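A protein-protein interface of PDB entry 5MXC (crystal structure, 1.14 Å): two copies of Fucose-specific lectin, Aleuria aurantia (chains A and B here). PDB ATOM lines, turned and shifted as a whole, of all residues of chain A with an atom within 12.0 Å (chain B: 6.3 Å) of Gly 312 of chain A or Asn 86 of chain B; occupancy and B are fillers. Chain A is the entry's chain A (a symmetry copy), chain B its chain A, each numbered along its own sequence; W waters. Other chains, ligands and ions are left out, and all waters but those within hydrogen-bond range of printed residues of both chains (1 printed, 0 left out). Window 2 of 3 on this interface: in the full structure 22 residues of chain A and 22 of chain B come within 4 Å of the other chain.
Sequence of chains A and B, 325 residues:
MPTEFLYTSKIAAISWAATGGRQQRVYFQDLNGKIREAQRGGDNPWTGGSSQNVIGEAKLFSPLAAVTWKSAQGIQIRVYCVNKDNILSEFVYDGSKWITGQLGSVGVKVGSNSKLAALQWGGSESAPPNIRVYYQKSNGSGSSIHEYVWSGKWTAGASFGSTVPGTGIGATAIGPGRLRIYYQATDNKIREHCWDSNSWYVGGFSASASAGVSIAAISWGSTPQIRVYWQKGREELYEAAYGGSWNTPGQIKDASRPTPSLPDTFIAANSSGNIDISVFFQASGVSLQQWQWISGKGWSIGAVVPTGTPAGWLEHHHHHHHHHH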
ATOM      1  N   PRO A   2      24.879   8.541  12.841  1.00  0.00           N
ATOM      2  CA  PRO A   2      24.543   9.694  12.016  1.00  0.00           C
ATOM      3  C   PRO A   2      23.718  10.681  12.804  1.00  0.00           C
ATOM      4  O   PRO A   2      23.259  10.385  13.912  1.00  0.00           O
ATOM      5  CB  PRO A   2      23.728   9.084  10.871  1.00  0.00           C
ATOM      6  CG  PRO A   2      23.156   7.831  11.418  1.00  0.00           C
ATOM      7  CD  PRO A   2      23.999   7.393  12.569  1.00  0.00           C
ATOM      8  N   THR A   3      23.521  11.861  12.214  1.00  0.00           N
ATOM      9  CA  THR A   3      22.700  12.905  12.838  1.00  0.00           C
ATOM     10  C   THR A   3      21.708  13.457  11.829  1.00  0.00           C
ATOM     11  O   THR A   3      21.682  13.029  10.678  1.00  0.00           O
ATOM     12  CB  THR A   3      23.570  14.064  13.366  1.00  0.00           C
ATOM     13  OG1 THR A   3      23.970  14.873  12.256  1.00  0.00           O
ATOM     14  CG2 THR A   3      24.794  13.562  14.135  1.00  0.00           C
ATOM     15  N   GLU A   4      20.923  14.432  12.271  1.00  0.00           N
ATOM     16  CA  GLU A   4      19.967  15.106  11.394  1.00  0.00           C
ATOM     17  C   GLU A   4      20.489  16.428  10.838  1.00  0.00           C
ATOM     18  O   GLU A   4      19.714  17.169  10.221  1.00  0.00           O
ATOM     19  CB  GLU A   4      18.634  15.254  12.136  1.00  0.00           C
ATOM     20  CG  GLU A   4      18.093  13.870  12.502  1.00  0.00           C
ATOM     21  CD  GLU A   4      16.841  13.872  13.335  1.00  0.00           C
ATOM     22  OE1 GLU A   4      16.713  14.729  14.233  1.00  0.00           O
ATOM     23  OE2 GLU A   4      15.972  12.992  13.092  1.00  0.00           O
ATOM     24  N   LEU A  31      17.582  17.656   7.810  1.00  0.00           N
ATOM     25  CA  LEU A  31      17.352  16.926   6.549  1.00  0.00           C
ATOM     26  C   LEU A  31      16.022  17.249   5.910  1.00  0.00           C
ATOM     27  O   LEU A  31      15.871  17.079   4.700  1.00  0.00           O
ATOM     28  CB  LEU A  31      17.441  15.408   6.786  1.00  0.00           C
ATOM     29  CG  LEU A  31      18.754  14.918   7.384  1.00  0.00           C
ATOM     30  CD1 LEU A  31      18.661  13.428   7.660  1.00  0.00           C
ATOM     31  CD2 LEU A  31      19.924  15.221   6.468  1.00  0.00           C
ATOM     32  N   SER A  51      14.406  17.561  16.738  1.00  0.00           N
ATOM     33  CA  SER A  51      13.183  17.885  16.013  1.00  0.00           C
ATOM     34  C   SER A  51      12.196  18.713  16.842  1.00  0.00           C
ATOM     35  O   SER A  51      11.279  19.293  16.278  1.00  0.00           O
ATOM     36  CB  SER A  51      12.502  16.610  15.521  1.00  0.00           C
ATOM     37  OG  SER A  51      12.052  15.857  16.616  1.00  0.00           O
ATOM     38  N   GLY A 308      20.544  16.100  16.663  1.00  0.00           N
ATOM     39  CA  GLY A 308      19.538  15.073  16.460  1.00  0.00           C
ATOM     40  C   GLY A 308      20.111  13.718  16.135  1.00  0.00           C
ATOM     41  O   GLY A 308      21.266  13.586  15.738  1.00  0.00           O
ATOM     42  N   THR A 309      19.265  12.706  16.284  1.00  0.00           N
ATOM     43  CA  THR A 309      19.595  11.330  15.926  1.00  0.00           C
ATOM     44  C   THR A 309      18.402  10.760  15.167  1.00  0.00           C
ATOM     45  O   THR A 309      17.295  10.763  15.698  1.00  0.00           O
ATOM     46  CB  THR A 309      19.860  10.462  17.166  1.00  0.00           C
ATOM     47  OG1 THR A 309      20.923  11.040  17.928  1.00  0.00           O
ATOM     48  CG2 THR A 309      20.269   9.053  16.775  1.00  0.00           C
ATOM     49  N   PRO A 310      18.603  10.284  13.920  1.00  0.00           N
ATOM     50  CA  PRO A 310      17.476   9.738  13.169  1.00  0.00           C
ATOM     51  C   PRO A 310      16.911   8.471  13.821  1.00  0.00           C
ATOM     52  O   PRO A 310      17.627   7.748  14.497  1.00  0.00           O
ATOM     53  CB  PRO A 310      18.075   9.452  11.787  1.00  0.00           C
ATOM     54  CG  PRO A 310      19.539   9.318  12.008  1.00  0.00           C
ATOM     55  CD  PRO A 310      19.893  10.092  13.236  1.00  0.00           C
ATOM     56  N   ALA A 311      15.636   8.220  13.574  1.00  0.00           N
ATOM     57  CA  ALA A 311      14.999   6.985  14.018  1.00  0.00           C
ATOM     58  C   ALA A 311      15.755   5.772  13.463  1.00  0.00           C
ATOM     59  O   ALA A 311      16.217   5.764  12.307  1.00  0.00           O
ATOM     60  CB  ALA A 311      13.554   6.956  13.565  1.00  0.00           C
ATOM     61  N   GLY A 312      15.883   4.752  14.297  1.00  0.00           N
ATOM     62  CA  GLY A 312      16.615   3.552  13.940  1.00  0.00           C
ATOM     63  C   GLY A 312      18.073   3.565  14.328  1.00  0.00           C
ATOM     64  O   GLY A 312      18.814   2.642  13.989  1.00  0.00           O
ATOM     65  N   TRP A 313      18.492   4.617  15.028  1.00  0.00           N
ATOM     66  CA  TRP A 313      19.865   4.780  15.467  1.00  0.00           C
ATOM     67  C   TRP A 313      19.839   5.242  16.922  1.00  0.00           C
ATOM     68  O   TRP A 313      18.839   5.815  17.373  1.00  0.00           O
ATOM     69  CB  TRP A 313      20.565   5.837  14.621  1.00  0.00           C
ATOM     70  CG  TRP A 313      20.708   5.480  13.188  1.00  0.00           C
ATOM     71  CD1 TRP A 313      19.823   5.729  12.192  1.00  0.00           C
ATOM     72  CD2 TRP A 313      21.813   4.790  12.592  1.00  0.00           C
ATOM     73  NE1 TRP A 313      20.314   5.251  11.000  1.00  0.00           N
ATOM     74  CE2 TRP A 313      21.535   4.666  11.218  1.00  0.00           C
ATOM     75  CE3 TRP A 313      23.018   4.277  13.092  1.00  0.00           C
ATOM     76  CZ2 TRP A 313      22.444   4.078  10.323  1.00  0.00           C
ATOM     77  CZ3 TRP A 313      23.908   3.696  12.216  1.00  0.00           C
ATOM     78  CH2 TRP A 313      23.622   3.612  10.848  1.00  0.00           C
ATOM     79  N   LEU A 314      20.934   5.023  17.641  1.00  0.00           N
ATOM     80  CA  LEU A 314      21.065   5.529  19.029  1.00  0.00           C
ATOM     81  C   LEU A 314      22.116   6.623  19.088  1.00  0.00           C
ATOM     82  O   LEU A 314      23.017   6.667  18.253  1.00  0.00           O
ATOM     83  CB  LEU A 314      21.408   4.396  20.004  1.00  0.00           C
ATOM     84  CG  LEU A 314      20.234   3.670  20.661  1.00  0.00           C
ATOM     85  CD1 LEU A 314      19.090   3.409  19.697  1.00  0.00           C
ATOM     86  CD2 LEU A 314      20.714   2.373  21.302  1.00  0.00           C
ATOM     87  N   LYS B  59      14.771   3.573   6.930  1.00  0.00           N
ATOM     88  CA  LYS B  59      15.307   4.501   7.919  1.00  0.00           C
ATOM     89  C   LYS B  59      16.372   5.367   7.261  1.00  0.00           C
ATOM     90  O   LYS B  59      17.049   4.944   6.303  1.00  0.00           O
ATOM     91  CB  LYS B  59      15.904   3.780   9.136  1.00  0.00           C
ATOM     92  CG  LYS B  59      17.254   3.099   8.927  1.00  0.00           C
ATOM     93  CD  LYS B  59      17.833   2.599  10.230  1.00  0.00           C
ATOM     94  CE  LYS B  59      19.239   2.050  10.075  1.00  0.00           C
ATOM     95  NZ  LYS B  59      19.798   1.724  11.422  1.00  0.00           N
ATOM     96  N   VAL B  82      16.511  -1.455   5.607  1.00  0.00           N
ATOM     97  CA  VAL B  82      15.904  -1.672   6.934  1.00  0.00           C
ATOM     98  C   VAL B  82      15.036  -0.512   7.289  1.00  0.00           C
ATOM     99  O   VAL B  82      15.257   0.658   6.903  1.00  0.00           O
ATOM    100  CB  VAL B  82      16.862  -1.905   8.125  1.00  0.00           C
ATOM    101  CG1 VAL B  82      17.898  -2.966   7.798  1.00  0.00           C
ATOM    102  CG2 VAL B  82      17.498  -0.602   8.587  1.00  0.00           C
ATOM    103  N   ASN B  83      13.978  -0.856   8.015  1.00  0.00           N
ATOM    104  CA  ASN B  83      13.000   0.150   8.419  1.00  0.00           C
ATOM    105  C   ASN B  83      13.436   0.857   9.707  1.00  0.00           C
ATOM    106  O   ASN B  83      14.519   0.625  10.224  1.00  0.00           O
ATOM    107  CB  ASN B  83      11.589  -0.453   8.451  1.00  0.00           C
ATOM    108  CG  ASN B  83      11.334  -1.353   9.646  1.00  0.00           C
ATOM    109  OD1 ASN B  83      12.142  -1.461  10.566  1.00  0.00           O
ATOM    110  ND2 ASN B  83      10.174  -2.011   9.637  1.00  0.00           N
ATOM    111  N   LYS B  84      12.553   1.724  10.222  1.00  0.00           N
ATOM    112  CA  LYS B  84      12.876   2.558  11.383  1.00  0.00           C
ATOM    113  C   LYS B  84      12.993   1.746  12.682  1.00  0.00           C
ATOM    114  O   LYS B  84      13.514   2.251  13.669  1.00  0.00           O
ATOM    115  CB  LYS B  84      11.848   3.687  11.553  1.00  0.00           C
ATOM    116  CG  LYS B  84      11.669   4.572  10.320  1.00  0.00           C
ATOM    117  CD  LYS B  84      12.587   5.777  10.301  1.00  0.00           C
ATOM    118  CE  LYS B  84      12.094   6.825   9.328  1.00  0.00           C
ATOM    119  NZ  LYS B  84      11.069   7.733   9.930  1.00  0.00           N
ATOM    120  N   ASP B  85      12.507   0.500  12.663  1.00  0.00           N
ATOM    121  CA  ASP B  85      12.651  -0.442  13.777  1.00  0.00           C
ATOM    122  C   ASP B  85      13.802  -1.426  13.547  1.00  0.00           C
ATOM    123  O   ASP B  85      13.930  -2.426  14.253  1.00  0.00           O
ATOM    124  CB  ASP B  85      11.319  -1.156  14.012  1.00  0.00           C
ATOM    125  CG  ASP B  85      10.231  -0.194  14.487  1.00  0.00           C
ATOM    126  OD1 ASP B  85      10.529   0.604  15.387  1.00  0.00           O
ATOM    127  OD2 ASP B  85       9.125  -0.225  13.937  1.00  0.00           O
ATOM    128  N   ASN B  86      14.668  -1.121  12.582  1.00  0.00           N
ATOM    129  CA  ASN B  86      15.798  -1.987  12.251  1.00  0.00           C
ATOM    130  C   ASN B  86      15.394  -3.392  11.838  1.00  0.00           C
ATOM    131  O   ASN B  86      16.091  -4.365  12.116  1.00  0.00           O
ATOM    132  CB  ASN B  86      16.847  -1.985  13.363  1.00  0.00           C
ATOM    133  CG  ASN B  86      17.664  -0.714  13.348  1.00  0.00           C
ATOM    134  OD1 ASN B  86      18.225  -0.350  12.300  1.00  0.00           O
ATOM    135  ND2 ASN B  86      17.740  -0.021  14.482  1.00  0.00           N
ATOM    136  N   ILE B  87      14.257  -3.487  11.153  1.00  0.00           N
ATOM    137  CA  ILE B  87      13.804  -4.760  10.611  1.00  0.00           C
ATOM    138  C   ILE B  87      14.161  -4.817   9.129  1.00  0.00           C
ATOM    139  O   ILE B  87      13.850  -3.893   8.362  1.00  0.00           O
ATOM    140  CB  ILE B  87      12.289  -4.965  10.826  1.00  0.00           C
ATOM    141  CG1 ILE B  87      11.924  -4.955  12.328  1.00  0.00           C
ATOM    142  CG2 ILE B  87      11.819  -6.251  10.160  1.00  0.00           C
ATOM    143  CD1 ILE B  87      12.578  -6.015  13.163  1.00  0.00           C
ATOM    144  N   LEU B  88      14.795  -5.918   8.740  1.00  0.00           N
ATOM    145  CA  LEU B  88      15.187  -6.176   7.356  1.00  0.00           C
ATOM    146  C   LEU B  88      13.957  -6.176   6.466  1.00  0.00           C
ATOM    147  O   LEU B  88      12.980  -6.889   6.747  1.00  0.00           O
ATOM    148  CB  LEU B  88      15.922  -7.511   7.304  1.00  0.00           C
ATOM    149  CG  LEU B  88      16.525  -7.919   5.964  1.00  0.00           C
ATOM    150  CD1 LEU B  88      17.536  -6.904   5.440  1.00  0.00           C
ATOM    151  CD2 LEU B  88      17.151  -9.298   6.088  1.00  0.00           C
ATOM    152  N   VAL B 108      13.303 -10.081  10.878  1.00  0.00           N
ATOM    153  CA  VAL B 108      14.755 -10.191  11.038  1.00  0.00           C
ATOM    154  C   VAL B 108      15.302  -8.852  11.542  1.00  0.00           C
ATOM    155  O   VAL B 108      15.290  -7.849  10.803  1.00  0.00           O
ATOM    156  CB  VAL B 108      15.432 -10.574   9.709  1.00  0.00           C
ATOM    157  CG1 VAL B 108      16.948 -10.663   9.894  1.00  0.00           C
ATOM    158  CG2 VAL B 108      14.859 -11.880   9.157  1.00  0.00           C
ATOM    159  N   LYS B 109      15.758  -8.830  12.792  1.00  0.00           N
ATOM    160  CA  LYS B 109      16.386  -7.651  13.372  1.00  0.00           C
ATOM    161  C   LYS B 109      17.802  -7.510  12.860  1.00  0.00           C
ATOM    162  O   LYS B 109      18.532  -8.502  12.732  1.00  0.00           O
ATOM    163  CB  LYS B 109      16.440  -7.748  14.886  1.00  0.00           C
ATOM    164  CG  LYS B 109      15.092  -7.799  15.566  1.00  0.00           C
ATOM    165  CD  LYS B 109      15.339  -8.212  16.991  1.00  0.00           C
ATOM    166  CE  LYS B 109      14.353  -7.596  17.934  1.00  0.00           C
ATOM    167  NZ  LYS B 109      14.864  -7.757  19.312  1.00  0.00           N
ATOM    168  N   VAL B 110      18.165  -6.268  12.545  1.00  0.00           N
ATOM    169  CA  VAL B 110      19.474  -5.926  12.002  1.00  0.00           C
ATOM    170  C   VAL B 110      20.154  -4.954  12.981  1.00  0.00           C
ATOM    171  O   VAL B 110      19.483  -4.054  13.504  1.00  0.00           O
ATOM    172  CB  VAL B 110      19.280  -5.327  10.585  1.00  0.00           C
ATOM    173  CG1 VAL B 110      20.619  -4.986   9.955  1.00  0.00           C
ATOM    174  CG2 VAL B 110      18.518  -6.315   9.695  1.00  0.00           C
ATOM    175  N   GLY B 111      21.460  -5.090  13.194  1.00  0.00           N
ATOM    176  CA  GLY B 111      22.201  -4.100  13.981  1.00  0.00           C
ATOM    177  C   GLY B 111      22.098  -2.735  13.318  1.00  0.00           C
ATOM    178  O   GLY B 111      22.090  -2.630  12.075  1.00  0.00           O
ATOM    179  N   SER B 112      22.007  -1.673  14.113  1.00  0.00           N
ATOM    180  CA  SER B 112      21.734  -0.362  13.537  1.00  0.00           C
ATOM    181  C   SER B 112      22.789   0.078  12.519  1.00  0.00           C
ATOM    182  O   SER B 112      22.423   0.755  11.554  1.00  0.00           O
ATOM    183  CB  SER B 112      21.570   0.689  14.633  1.00  0.00           C
ATOM    184  OG  SER B 112      22.769   0.824  15.349  1.00  0.00           O
ATOM    185  N   ASN B 113      24.052  -0.304  12.727  1.00  0.00           N
ATOM    186  CA  ASN B 113      25.130   0.068  11.817  1.00  0.00           C
ATOM    187  C   ASN B 113      25.498  -1.036  10.820  1.00  0.00           C
ATOM    188  O   ASN B 113      26.530  -0.932  10.148  1.00  0.00           O
ATOM    189  CB  ASN B 113      26.372   0.480  12.608  1.00  0.00           C
ATOM    190  CG  ASN B 113      27.353   1.291  11.779  1.00  0.00           C
ATOM    191  OD1 ASN B 113      26.955   2.130  10.974  1.00  0.00           O
ATOM    192  ND2 ASN B 113      28.637   1.053  11.979  1.00  0.00           N
HETATM  193  O   HOH W   1      23.028   3.130  16.779  1.00  0.00           O
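The backbone carbonyl oxygen of Gly 312 of chain A is in hydrogen-bond range of the side-chain amide nitrogen of Asn 86 of chain B. The side-chain amino group (NZ) of Lys 59 of chain B lies within hydrogen-bond range of the backbone carbonyl oxygen (O) of Gly 312 of chain A (2.9 Å).
The side-chain amino group of Lys 59 of chain B sits at hydrogen-bond distance from the side-chain amide oxygen of Asn 86 of chain B, at 2.7 Å. The backbone NH of Asn 86 of chain B lies within hydrogen-bond range of the side-chain amide oxygen of Asn 83 of chain B. The side-chain amino group of Lys 59 of chain B lies within hydrogen-bond range of the backbone carbonyl oxygen of Ser 112 of chain B (2.8 Å). The backbone NH (N) of Lys 59 of chain B sits at hydrogen-bond distance from the backbone carbonyl oxygen (O) of Val 82 of chain B (3.0 Å). O of Asn 86 of chain B lies within hydrogen-bond range of N of Val 110 of chain B, at 2.8 Å.
Lys 59 of chain B touches Ala 311 of chain A (CB to O, 3.8 Å). Lys 84 of chain B touches Ala 311 of chain A (CD to CB, 3.6 Å). Lys 84 of chain B touches Gly 312 of chain A (O to CA, 3.4 Å). O of Gly 312 of chain A touches CB of Ser 112 of chain B, at 3.4 Å. Lys 59 of chain B touches Trp 313 of chain A (NZ to CE2, 3.4 Å). Trp 313 of chain A touches Ser 112 of chain B. OD1 of Asn 113 of chain B touches CZ3 of Trp 313 of chain A (3.6 Å).
Of the printed residues of chain B, Gly 312 of chain A touches Lys 59, Lys 84, Asn 86 and Ser 112. Printed residues of chain A within 4 Å of Asn 86 of chain B: Gly 312. Lys 59 of chain B touches just these residues of chain A: Ala 311, Gly 312 and Trp 313. No residue of chain A comes within 4 Å of Asp 85 of chain B. No residue of chain A comes within 4 Å of Ile 87 of chain B. No residue of chain A comes within 4 Å of Gly 111 of chain B. Printed residues of chain B within 4 Å of Ala 311 of chain A: Lys 59 (3.8 Å) and Lys 84 (3.6 Å). Of the printed residues of chain B, Trp 313 of chain A touches Lys 59, Ser 112 and Asn 113. The nearest printed residue of chain B that does not touch Gly 312 of chain A is Asn 83 of chain B (5.2 Å). The nearest residue of chain A that does not touch Asn 86 of chain B is Trp 313 of chain A (4.7 Å).
Of the 12 printed residues of chain A, 3 touch a printed residue of chain B. Among the printed residues, no Asp or Glu carboxylate lies within 4 Å of a Lys or Arg side-chain nitrogen of the other chain.
No position is printed for both chains.
Water W1 bridges the side-chain hydroxyl of Ser 112 of chain B (2.7 Å) and the backbone NH of Leu 314 of chain A (3.0 Å).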
